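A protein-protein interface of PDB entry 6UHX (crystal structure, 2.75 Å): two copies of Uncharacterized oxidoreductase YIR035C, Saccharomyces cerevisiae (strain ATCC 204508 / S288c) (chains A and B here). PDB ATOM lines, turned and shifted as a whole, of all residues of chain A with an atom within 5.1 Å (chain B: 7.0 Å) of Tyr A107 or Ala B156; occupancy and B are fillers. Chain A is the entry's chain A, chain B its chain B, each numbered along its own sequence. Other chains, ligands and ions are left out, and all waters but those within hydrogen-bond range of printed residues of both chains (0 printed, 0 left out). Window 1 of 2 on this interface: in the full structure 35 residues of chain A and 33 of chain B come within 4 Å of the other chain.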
ATOM      1  N   TRP A 103      26.250   2.824  -3.375  1.00  0.00           N
ATOM      2  CA  TRP A 103      25.531   3.219  -4.582  1.00  0.00           C
ATOM      3  C   TRP A 103      26.338   2.899  -5.833  1.00  0.00           C
ATOM      4  O   TRP A 103      25.785   2.421  -6.830  1.00  0.00           O
ATOM      5  CB  TRP A 103      25.195   4.710  -4.528  1.00  0.00           C
ATOM      6  CG  TRP A 103      23.975   5.034  -3.718  1.00  0.00           C
ATOM      7  CD1 TRP A 103      23.695   4.608  -2.452  1.00  0.00           C
ATOM      8  CD2 TRP A 103      22.874   5.858  -4.117  1.00  0.00           C
ATOM      9  NE1 TRP A 103      22.487   5.114  -2.039  1.00  0.00           N
ATOM     10  CE2 TRP A 103      21.962   5.885  -3.043  1.00  0.00           C
ATOM     11  CE3 TRP A 103      22.569   6.575  -5.279  1.00  0.00           C
ATOM     12  CZ2 TRP A 103      20.767   6.601  -3.096  1.00  0.00           C
ATOM     13  CZ3 TRP A 103      21.382   7.285  -5.329  1.00  0.00           C
ATOM     14  CH2 TRP A 103      20.497   7.292  -4.244  1.00  0.00           C
ATOM     15  N   LYS A 104      27.648   3.164  -5.803  1.00  0.00           N
ATOM     16  CA  LYS A 104      28.497   2.823  -6.940  1.00  0.00           C
ATOM     17  C   LYS A 104      28.573   1.314  -7.132  1.00  0.00           C
ATOM     18  O   LYS A 104      28.642   0.828  -8.268  1.00  0.00           O
ATOM     19  CB  LYS A 104      29.894   3.412  -6.746  1.00  0.00           C
ATOM     20  CG  LYS A 104      29.898   4.870  -6.322  1.00  0.00           C
ATOM     21  CD  LYS A 104      31.313   5.388  -6.132  1.00  0.00           C
ATOM     22  CE  LYS A 104      31.311   6.797  -5.559  1.00  0.00           C
ATOM     23  NZ  LYS A 104      32.688   7.347  -5.433  1.00  0.00           N
ATOM     24  N   LYS A 105      28.565   0.558  -6.033  1.00  0.00           N
ATOM     25  CA  LYS A 105      28.507  -0.897  -6.127  1.00  0.00           C
ATOM     26  C   LYS A 105      27.206  -1.350  -6.776  1.00  0.00           C
ATOM     27  O   LYS A 105      27.184  -2.331  -7.529  1.00  0.00           O
ATOM     28  CB  LYS A 105      28.668  -1.506  -4.735  1.00  0.00           C
ATOM     29  CG  LYS A 105      28.656  -3.023  -4.689  1.00  0.00           C
ATOM     30  CD  LYS A 105      28.242  -3.519  -3.308  1.00  0.00           C
ATOM     31  CE  LYS A 105      27.241  -2.573  -2.651  1.00  0.00           C
ATOM     32  NZ  LYS A 105      27.102  -2.818  -1.188  1.00  0.00           N
ATOM     33  N   LEU A 106      26.108  -0.643  -6.493  1.00  0.00           N
ATOM     34  CA  LEU A 106      24.850  -0.899  -7.186  1.00  0.00           C
ATOM     35  C   LEU A 106      24.949  -0.514  -8.657  1.00  0.00           C
ATOM     36  O   LEU A 106      24.461  -1.241  -9.531  1.00  0.00           O
ATOM     37  CB  LEU A 106      23.721  -0.131  -6.492  1.00  0.00           C
ATOM     38  CG  LEU A 106      22.271  -0.117  -6.999  1.00  0.00           C
ATOM     39  CD1 LEU A 106      22.057   0.973  -8.047  1.00  0.00           C
ATOM     40  CD2 LEU A 106      21.817  -1.472  -7.519  1.00  0.00           C
ATOM     41  N   TYR A 107      25.581   0.626  -8.950  1.00  0.00           N
ATOM     42  CA  TYR A 107      25.714   1.085 -10.326  1.00  0.00           C
ATOM     43  C   TYR A 107      26.692   0.240 -11.130  1.00  0.00           C
ATOM     44  O   TYR A 107      26.590   0.199 -12.361  1.00  0.00           O
ATOM     45  CB  TYR A 107      26.156   2.549 -10.351  1.00  0.00           C
ATOM     46  CG  TYR A 107      25.017   3.528 -10.496  1.00  0.00           C
ATOM     47  CD1 TYR A 107      24.157   3.786  -9.436  1.00  0.00           C
ATOM     48  CD2 TYR A 107      24.798   4.195 -11.694  1.00  0.00           C
ATOM     49  CE1 TYR A 107      23.113   4.680  -9.564  1.00  0.00           C
ATOM     50  CE2 TYR A 107      23.756   5.091 -11.832  1.00  0.00           C
ATOM     51  CZ  TYR A 107      22.917   5.329 -10.764  1.00  0.00           C
ATOM     52  OH  TYR A 107      21.880   6.222 -10.898  1.00  0.00           O
ATOM     53  N   ASP A 108      27.635  -0.430 -10.470  1.00  0.00           N
ATOM     54  CA  ASP A 108      28.604  -1.264 -11.166  1.00  0.00           C
ATOM     55  C   ASP A 108      28.014  -2.581 -11.650  1.00  0.00           C
ATOM     56  O   ASP A 108      28.680  -3.296 -12.406  1.00  0.00           O
ATOM     57  CB  ASP A 108      29.803  -1.545 -10.255  1.00  0.00           C
ATOM     58  CG  ASP A 108      31.117  -1.580 -11.011  1.00  0.00           C
ATOM     59  OD1 ASP A 108      31.095  -1.828 -12.235  1.00  0.00           O
ATOM     60  OD2 ASP A 108      32.172  -1.360 -10.382  1.00  0.00           O
ATOM     61  N   ILE A 109      26.792  -2.917 -11.244  1.00  0.00           N
ATOM     62  CA  ILE A 109      26.164  -4.177 -11.606  1.00  0.00           C
ATOM     63  C   ILE A 109      25.027  -3.976 -12.602  1.00  0.00           C
ATOM     64  O   ILE A 109      24.887  -4.754 -13.549  1.00  0.00           O
ATOM     65  CB  ILE A 109      25.665  -4.922 -10.347  1.00  0.00           C
ATOM     66  CG1 ILE A 109      26.787  -5.035  -9.314  1.00  0.00           C
ATOM     67  CG2 ILE A 109      25.131  -6.298 -10.715  1.00  0.00           C
ATOM     68  CD1 ILE A 109      26.423  -5.854  -8.095  1.00  0.00           C
ATOM     69  N   ASN A 110      24.211  -2.942 -12.411  1.00  0.00           N
ATOM     70  CA  ASN A 110      23.035  -2.732 -13.243  1.00  0.00           C
ATOM     71  C   ASN A 110      23.264  -1.747 -14.383  1.00  0.00           C
ATOM     72  O   ASN A 110      22.395  -1.624 -15.252  1.00  0.00           O
ATOM     73  CB  ASN A 110      21.861  -2.240 -12.390  1.00  0.00           C
ATOM     74  CG  ASN A 110      21.632  -3.094 -11.160  1.00  0.00           C
ATOM     75  OD1 ASN A 110      22.392  -4.020 -10.883  1.00  0.00           O
ATOM     76  ND2 ASN A 110      20.580  -2.783 -10.412  1.00  0.00           N
ATOM     77  N   PHE A 111      24.396  -1.045 -14.405  1.00  0.00           N
ATOM     78  CA  PHE A 111      24.646  -0.071 -15.459  1.00  0.00           C
ATOM     79  C   PHE A 111      26.059  -0.198 -16.013  1.00  0.00           C
ATOM     80  O   PHE A 111      26.241  -0.494 -17.197  1.00  0.00           O
ATOM     81  CB  PHE A 111      24.406   1.349 -14.943  1.00  0.00           C
ATOM     82  CG  PHE A 111      24.628   2.414 -15.979  1.00  0.00           C
ATOM     83  CD1 PHE A 111      23.738   2.574 -17.026  1.00  0.00           C
ATOM     84  CD2 PHE A 111      25.729   3.251 -15.907  1.00  0.00           C
ATOM     85  CE1 PHE A 111      23.940   3.552 -17.983  1.00  0.00           C
ATOM     86  CE2 PHE A 111      25.937   4.230 -16.860  1.00  0.00           C
ATOM     87  CZ  PHE A 111      25.040   4.381 -17.898  1.00  0.00           C
ATOM     88  N   PHE A 112      27.064   0.027 -15.162  1.00  0.00           N
ATOM     89  CA  PHE A 112      28.449  -0.040 -15.617  1.00  0.00           C
ATOM     90  C   PHE A 112      28.821  -1.438 -16.093  1.00  0.00           C
ATOM     91  O   PHE A 112      29.688  -1.587 -16.961  1.00  0.00           O
ATOM     92  CB  PHE A 112      29.389   0.410 -14.499  1.00  0.00           C
ATOM     93  CG  PHE A 112      29.284   1.871 -14.172  1.00  0.00           C
ATOM     94  CD1 PHE A 112      29.123   2.809 -15.179  1.00  0.00           C
ATOM     95  CD2 PHE A 112      29.344   2.308 -12.859  1.00  0.00           C
ATOM     96  CE1 PHE A 112      29.024   4.155 -14.883  1.00  0.00           C
ATOM     97  CE2 PHE A 112      29.246   3.652 -12.556  1.00  0.00           C
ATOM     98  CZ  PHE A 112      29.086   4.578 -13.569  1.00  0.00           C
ATOM     99  N   SER A 113      28.180  -2.470 -15.540  1.00  0.00           N
ATOM    100  CA  SER A 113      28.421  -3.828 -16.016  1.00  0.00           C
ATOM    101  C   SER A 113      27.917  -4.022 -17.438  1.00  0.00           C
ATOM    102  O   SER A 113      28.508  -4.790 -18.205  1.00  0.00           O
ATOM    103  CB  SER A 113      27.759  -4.839 -15.083  1.00  0.00           C
ATOM    104  OG  SER A 113      27.396  -6.012 -15.792  1.00  0.00           O
ATOM    105  N   ALA A 149      18.891   4.524  -5.355  1.00  0.00           N
ATOM    106  CA  ALA A 149      19.961   3.954  -6.164  1.00  0.00           C
ATOM    107  C   ALA A 149      19.398   3.096  -7.291  1.00  0.00           C
ATOM    108  O   ALA A 149      19.781   3.252  -8.454  1.00  0.00           O
ATOM    109  CB  ALA A 149      20.907   3.140  -5.283  1.00  0.00           C
ATOM    110  N   SER A 152      17.158   5.321 -10.108  1.00  0.00           N
ATOM    111  CA  SER A 152      18.030   5.999 -11.058  1.00  0.00           C
ATOM    112  C   SER A 152      18.974   5.041 -11.772  1.00  0.00           C
ATOM    113  O   SER A 152      19.570   5.425 -12.784  1.00  0.00           O
ATOM    114  CB  SER A 152      18.838   7.086 -10.348  1.00  0.00           C
ATOM    115  OG  SER A 152      19.638   6.533  -9.318  1.00  0.00           O
ATOM    116  N   SER A 153      19.129   3.816 -11.265  1.00  0.00           N
ATOM    117  CA  SER A 153      19.952   2.825 -11.948  1.00  0.00           C
ATOM    118  C   SER A 153      19.374   2.475 -13.313  1.00  0.00           C
ATOM    119  O   SER A 153      20.097   2.425 -14.314  1.00  0.00           O
ATOM    120  CB  SER A 153      20.086   1.574 -11.081  1.00  0.00           C
ATOM    121  OG  SER A 153      20.637   0.503 -11.821  1.00  0.00           O
ATOM    122  N   ALA A 155      17.054   4.273 -14.911  1.00  0.00           N
ATOM    123  CA  ALA A 155      16.879   5.485 -15.704  1.00  0.00           C
ATOM    124  C   ALA A 155      18.093   5.739 -16.588  1.00  0.00           C
ATOM    125  O   ALA A 155      17.955   6.180 -17.735  1.00  0.00           O
ATOM    126  CB  ALA A 155      16.619   6.682 -14.789  1.00  0.00           C
ATOM    127  N   ALA A 156      19.293   5.467 -16.069  1.00  0.00           N
ATOM    128  CA  ALA A 156      20.493   5.573 -16.891  1.00  0.00           C
ATOM    129  C   ALA A 156      20.547   4.472 -17.942  1.00  0.00           C
ATOM    130  O   ALA A 156      21.111   4.676 -19.023  1.00  0.00           O
ATOM    131  CB  ALA A 156      21.741   5.533 -16.010  1.00  0.00           C
ATOM    132  N   LYS B 104      32.947   6.280 -15.278  1.00  0.00           N
ATOM    133  CA  LYS B 104      32.659   6.368 -13.850  1.00  0.00           C
ATOM    134  C   LYS B 104      33.066   7.722 -13.283  1.00  0.00           C
ATOM    135  O   LYS B 104      32.333   8.308 -12.479  1.00  0.00           O
ATOM    136  CB  LYS B 104      33.368   5.241 -13.098  1.00  0.00           C
ATOM    137  CG  LYS B 104      32.863   3.846 -13.420  1.00  0.00           C
ATOM    138  CD  LYS B 104      33.180   2.885 -12.285  1.00  0.00           C
ATOM    139  CE  LYS B 104      33.657   1.539 -12.807  1.00  0.00           C
ATOM    140  NZ  LYS B 104      32.655   0.894 -13.698  1.00  0.00           N
ATOM    141  N   TYR B 107      30.454  10.109 -13.641  1.00  0.00           N
ATOM    142  CA  TYR B 107      29.395   9.860 -12.670  1.00  0.00           C
ATOM    143  C   TYR B 107      29.819  10.253 -11.262  1.00  0.00           C
ATOM    144  O   TYR B 107      28.984  10.695 -10.465  1.00  0.00           O
ATOM    145  CB  TYR B 107      28.987   8.387 -12.707  1.00  0.00           C
ATOM    146  CG  TYR B 107      27.876   8.079 -13.683  1.00  0.00           C
ATOM    147  CD1 TYR B 107      28.128   7.986 -15.045  1.00  0.00           C
ATOM    148  CD2 TYR B 107      26.575   7.877 -13.243  1.00  0.00           C
ATOM    149  CE1 TYR B 107      27.115   7.703 -15.942  1.00  0.00           C
ATOM    150  CE2 TYR B 107      25.555   7.594 -14.130  1.00  0.00           C
ATOM    151  CZ  TYR B 107      25.831   7.508 -15.478  1.00  0.00           C
ATOM    152  OH  TYR B 107      24.818   7.226 -16.365  1.00  0.00           O
ATOM    153  N   PHE B 111      27.190  12.956 -10.518  1.00  0.00           N
ATOM    154  CA  PHE B 111      26.136  12.215  -9.834  1.00  0.00           C
ATOM    155  C   PHE B 111      26.570  11.766  -8.444  1.00  0.00           C
ATOM    156  O   PHE B 111      25.937  12.124  -7.445  1.00  0.00           O
ATOM    157  CB  PHE B 111      25.711  11.005 -10.669  1.00  0.00           C
ATOM    158  CG  PHE B 111      24.616  10.190 -10.042  1.00  0.00           C
ATOM    159  CD1 PHE B 111      23.322  10.680  -9.975  1.00  0.00           C
ATOM    160  CD2 PHE B 111      24.879   8.932  -9.524  1.00  0.00           C
ATOM    161  CE1 PHE B 111      22.311   9.932  -9.400  1.00  0.00           C
ATOM    162  CE2 PHE B 111      23.873   8.180  -8.948  1.00  0.00           C
ATOM    163  CZ  PHE B 111      22.588   8.680  -8.886  1.00  0.00           C
ATOM    164  N   PHE B 112      27.649  10.982  -8.367  1.00  0.00           N
ATOM    165  CA  PHE B 112      28.054  10.419  -7.083  1.00  0.00           C
ATOM    166  C   PHE B 112      28.591  11.484  -6.136  1.00  0.00           C
ATOM    167  O   PHE B 112      28.505  11.323  -4.914  1.00  0.00           O
ATOM    168  CB  PHE B 112      29.086   9.314  -7.297  1.00  0.00           C
ATOM    169  CG  PHE B 112      28.518   8.078  -7.936  1.00  0.00           C
ATOM    170  CD1 PHE B 112      27.510   7.363  -7.310  1.00  0.00           C
ATOM    171  CD2 PHE B 112      28.986   7.635  -9.161  1.00  0.00           C
ATOM    172  CE1 PHE B 112      26.980   6.227  -7.893  1.00  0.00           C
ATOM    173  CE2 PHE B 112      28.461   6.499  -9.748  1.00  0.00           C
ATOM    174  CZ  PHE B 112      27.457   5.795  -9.113  1.00  0.00           C
ATOM    175  N   CYS B 140      19.138  14.670 -20.974  1.00  0.00           N
ATOM    176  CA  CYS B 140      18.467  13.612 -20.227  1.00  0.00           C
ATOM    177  C   CYS B 140      17.327  12.994 -21.028  1.00  0.00           C
ATOM    178  O   CYS B 140      17.005  11.817 -20.836  1.00  0.00           O
ATOM    179  CB  CYS B 140      17.947  14.156 -18.896  1.00  0.00           C
ATOM    180  SG  CYS B 140      16.622  15.374 -19.051  1.00  0.00           S
ATOM    181  N   GLY B 151      24.982  12.462 -21.028  1.00  0.00           N
ATOM    182  CA  GLY B 151      23.535  12.433 -21.122  1.00  0.00           C
ATOM    183  C   GLY B 151      22.887  11.451 -20.166  1.00  0.00           C
ATOM    184  O   GLY B 151      21.784  11.699 -19.670  1.00  0.00           O
ATOM    185  N   SER B 152      23.556  10.333 -19.889  1.00  0.00           N
ATOM    186  CA  SER B 152      22.996   9.325 -18.999  1.00  0.00           C
ATOM    187  C   SER B 152      23.160   9.689 -17.529  1.00  0.00           C
ATOM    188  O   SER B 152      22.369   9.235 -16.698  1.00  0.00           O
ATOM    189  CB  SER B 152      23.638   7.962 -19.274  1.00  0.00           C
ATOM    190  OG  SER B 152      25.025   8.089 -19.547  1.00  0.00           O
ATOM    191  N   SER B 153      24.158  10.509 -17.193  1.00  0.00           N
ATOM    192  CA  SER B 153      24.353  10.923 -15.807  1.00  0.00           C
ATOM    193  C   SER B 153      23.316  11.960 -15.387  1.00  0.00           C
ATOM    194  O   SER B 153      22.894  11.991 -14.223  1.00  0.00           O
ATOM    195  CB  SER B 153      25.760  11.485 -15.626  1.00  0.00           C
ATOM    196  OG  SER B 153      25.825  12.841 -16.021  1.00  0.00           O
ATOM    197  N   LYS B 154      22.907  12.832 -16.316  1.00  0.00           N
ATOM    198  CA  LYS B 154      21.831  13.772 -16.023  1.00  0.00           C
ATOM    199  C   LYS B 154      20.500  13.057 -15.838  1.00  0.00           C
ATOM    200  O   LYS B 154      19.662  13.512 -15.055  1.00  0.00           O
ATOM    201  CB  LYS B 154      21.720  14.813 -17.133  1.00  0.00           C
ATOM    202  CG  LYS B 154      22.936  15.717 -17.253  1.00  0.00           C
ATOM    203  CD  LYS B 154      23.184  16.475 -15.956  1.00  0.00           C
ATOM    204  CE  LYS B 154      24.407  17.376 -16.060  1.00  0.00           C
ATOM    205  NZ  LYS B 154      24.705  18.082 -14.780  1.00  0.00           N
ATOM    206  N   ALA B 155      20.290  11.940 -16.539  1.00  0.00           N
ATOM    207  CA  ALA B 155      19.059  11.176 -16.355  1.00  0.00           C
ATOM    208  C   ALA B 155      18.994  10.561 -14.962  1.00  0.00           C
ATOM    209  O   ALA B 155      17.912  10.457 -14.372  1.00  0.00           O
ATOM    210  CB  ALA B 155      18.949  10.097 -17.431  1.00  0.00           C
ATOM    211  N   ALA B 156      20.143  10.155 -14.419  1.00  0.00           N
ATOM    212  CA  ALA B 156      20.171   9.612 -13.066  1.00  0.00           C
ATOM    213  C   ALA B 156      20.016  10.707 -12.020  1.00  0.00           C
ATOM    214  O   ALA B 156      19.459  10.460 -10.946  1.00  0.00           O
ATOM    215  CB  ALA B 156      21.467   8.835 -12.835  1.00  0.00           C
ATOM    216  N   LEU B 157      20.501  11.916 -12.313  1.00  0.00           N
ATOM    217  CA  LEU B 157      20.352  13.022 -11.372  1.00  0.00           C
ATOM    218  C   LEU B 157      18.914  13.524 -11.318  1.00  0.00           C
ATOM    219  O   LEU B 157      18.444  13.935 -10.251  1.00  0.00           O
ATOM    220  CB  LEU B 157      21.300  14.161 -11.750  1.00  0.00           C
ATOM    221  CG  LEU B 157      21.381  15.340 -10.779  1.00  0.00           C
ATOM    222  CD1 LEU B 157      21.942  14.892  -9.438  1.00  0.00           C
ATOM    223  CD2 LEU B 157      22.223  16.461 -11.369  1.00  0.00           C
ATOM    224  N   ASN B 158      18.206  13.499 -12.449  1.00  0.00           N
ATOM    225  CA  ASN B 158      16.812  13.929 -12.458  1.00  0.00           C
ATOM    226  C   ASN B 158      15.942  13.000 -11.621  1.00  0.00           C
ATOM    227  O   ASN B 158      15.055  13.460 -10.894  1.00  0.00           O
ATOM    228  CB  ASN B 158      16.292  13.999 -13.894  1.00  0.00           C
ATOM    229  CG  ASN B 158      16.996  15.056 -14.715  1.00  0.00           C
ATOM    230  OD1 ASN B 158      17.973  15.655 -14.267  1.00  0.00           O
ATOM    231  ND2 ASN B 158      16.506  15.292 -15.926  1.00  0.00           N
ATOM    232  N   HIS B 159      16.181  11.690 -11.713  1.00  0.00           N
ATOM    233  CA  HIS B 159      15.432  10.746 -10.891  1.00  0.00           C
ATOM    234  C   HIS B 159      15.729  10.942  -9.411  1.00  0.00           C
ATOM    235  O   HIS B 159      14.851  10.729  -8.568  1.00  0.00           O
ATOM    236  CB  HIS B 159      15.752   9.311 -11.309  1.00  0.00           C
ATOM    237  CG  HIS B 159      15.133   8.274 -10.425  1.00  0.00           C
ATOM    238  ND1 HIS B 159      15.699   7.881  -9.230  1.00  0.00           N
ATOM    239  CD2 HIS B 159      13.996   7.550 -10.558  1.00  0.00           C
ATOM    240  CE1 HIS B 159      14.936   6.962  -8.665  1.00  0.00           C
ATOM    241  NE2 HIS B 159      13.897   6.742  -9.451  1.00  0.00           N
ATOM    242  N   PHE B 160      16.957  11.343  -9.077  1.00  0.00           N
ATOM    243  CA  PHE B 160      17.302  11.579  -7.681  1.00  0.00           C
ATOM    244  C   PHE B 160      16.594  12.808  -7.129  1.00  0.00           C
ATOM    245  O   PHE B 160      16.305  12.866  -5.928  1.00  0.00           O
ATOM    246  CB  PHE B 160      18.815  11.721  -7.531  1.00  0.00           C
ATOM    247  CG  PHE B 160      19.270  11.840  -6.107  1.00  0.00           C
ATOM    248  CD1 PHE B 160      19.153  10.768  -5.239  1.00  0.00           C
ATOM    249  CD2 PHE B 160      19.810  13.024  -5.636  1.00  0.00           C
ATOM    250  CE1 PHE B 160      19.568  10.874  -3.927  1.00  0.00           C
ATOM    251  CE2 PHE B 160      20.227  13.137  -4.325  1.00  0.00           C
ATOM    252  CZ  PHE B 160      20.105  12.058  -3.470  1.00  0.00           C
ATOM    253  N   ALA B 161      16.313  13.798  -7.980  1.00  0.00           N
ATOM    254  CA  ALA B 161      15.553  14.960  -7.534  1.00  0.00           C
ATOM    255  C   ALA B 161      14.137  14.569  -7.135  1.00  0.00           C
ATOM    256  O   ALA B 161      13.598  15.082  -6.147  1.00  0.00           O
ATOM    257  CB  ALA B 161      15.526  16.025  -8.629  1.00  0.00           C
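N of Ser A152 sits at hydrogen-bond distance from ND1 of His B159, 3.1 Å away. OD1 of Asp A108 is in salt-bridge range of NZ of Lys B104 (3.5 Å).
The side-chain hydroxyl of Tyr B107 is in hydrogen-bond range of the backbone carbonyl oxygen of Ser B152 (3.2 Å). The backbone carbonyl oxygen (O) of Tyr B107 is in hydrogen-bond range of the backbone NH (N) of Phe B112 (2.5 Å). The side-chain hydroxyl (OG) of Ser A152 sits at hydrogen-bond distance from the backbone carbonyl oxygen (O) of Ala A149, 3.4 Å away. The side-chain hydroxyl (OH) of Tyr B107 lies within hydrogen-bond range of the backbone NH (N) of Ser B153, at 3.4 Å. The backbone NH (N) of Phe A112 sits at hydrogen-bond distance from the backbone carbonyl oxygen (O) of Tyr A107 (2.8 Å). The backbone NH of Ser A113 sits close to the backbone carbonyl oxygen of Asp A108, at 3.3 Å.
Among the printed residues, pairs that only touch across the chains: Phe A111 with Tyr B107 (3.2 Å), Tyr A107 with Phe B111 (3.3 Å), Tyr A107 with Ala B156 (3.3 Å), Phe A112 with Lys B104 (3.4 Å), Ser A152 with Ala B156 (3.5 Å), Ala A156 with Tyr B107 (3.5 Å), Lys A104 with Phe B112 (3.6 Å), Tyr A107 with Phe B112 (3.6 Å), Ser A152 with Phe B111 (3.7 Å), Phe A112 with Tyr B107 (3.7 Å), Trp A103 with Phe B160 (3.7 Å), Ala A156 with Ser B152 (3.8 Å), Tyr A107 with Tyr B107 (3.8 Å) and Trp A103 with Phe B112 (3.97 Å).
Printed residues of chain B within 4 Å of Phe A112: Lys B104 and Tyr B107. Of the printed residues of chain A, Tyr B107 touches Tyr A107, Phe A111, Phe A112 and Ala A156. Printed residues of chain A within 4 Å of Phe B112: Trp A103 (3.97 Å), Lys A104 (3.6 Å) and Tyr A107 (3.6 Å). Ala B156 touches two residues of chain A. Printed residues of chain A within 4 Å of His B159: Ser A152 (3.1 Å). The nearest residue of chain B that does not touch Tyr A107 is Leu B157 (6.0 Å).
Hydrophobic or aromatic side chains of chain A within 4 Å of the printed part of chain B: Trp A103, Tyr A107, Phe A111, Phe A112 and Ala A156. Of the 16 printed residues of chain B, 8 touch a printed residue of chain A. Printed residues of chain B that touch a printed residue of chain A: Lys B104, Tyr B107, Phe B111, Phe B112, Ser B152, Ala B156, His B159 and Phe B160.
Tyr A107 touches its own counterpart, Tyr B107. Tyr A107 touches Phe B111, and with the chains exchanged Phe A111 touches Tyr B107. Tyr A107 touches Ala B156, and with the chains exchanged Ala A156 touches Tyr B107. Ser A152 touches Ala B156, and with the chains exchanged Ala A156 touches Ser B152. Positions printed for both chains: 104, 107, 111, 112, 152, 153, 155 and 156. Of the 16 pairs that touch across the chains among the printed residues, 11 have their exchanged pair printed and touching as well.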
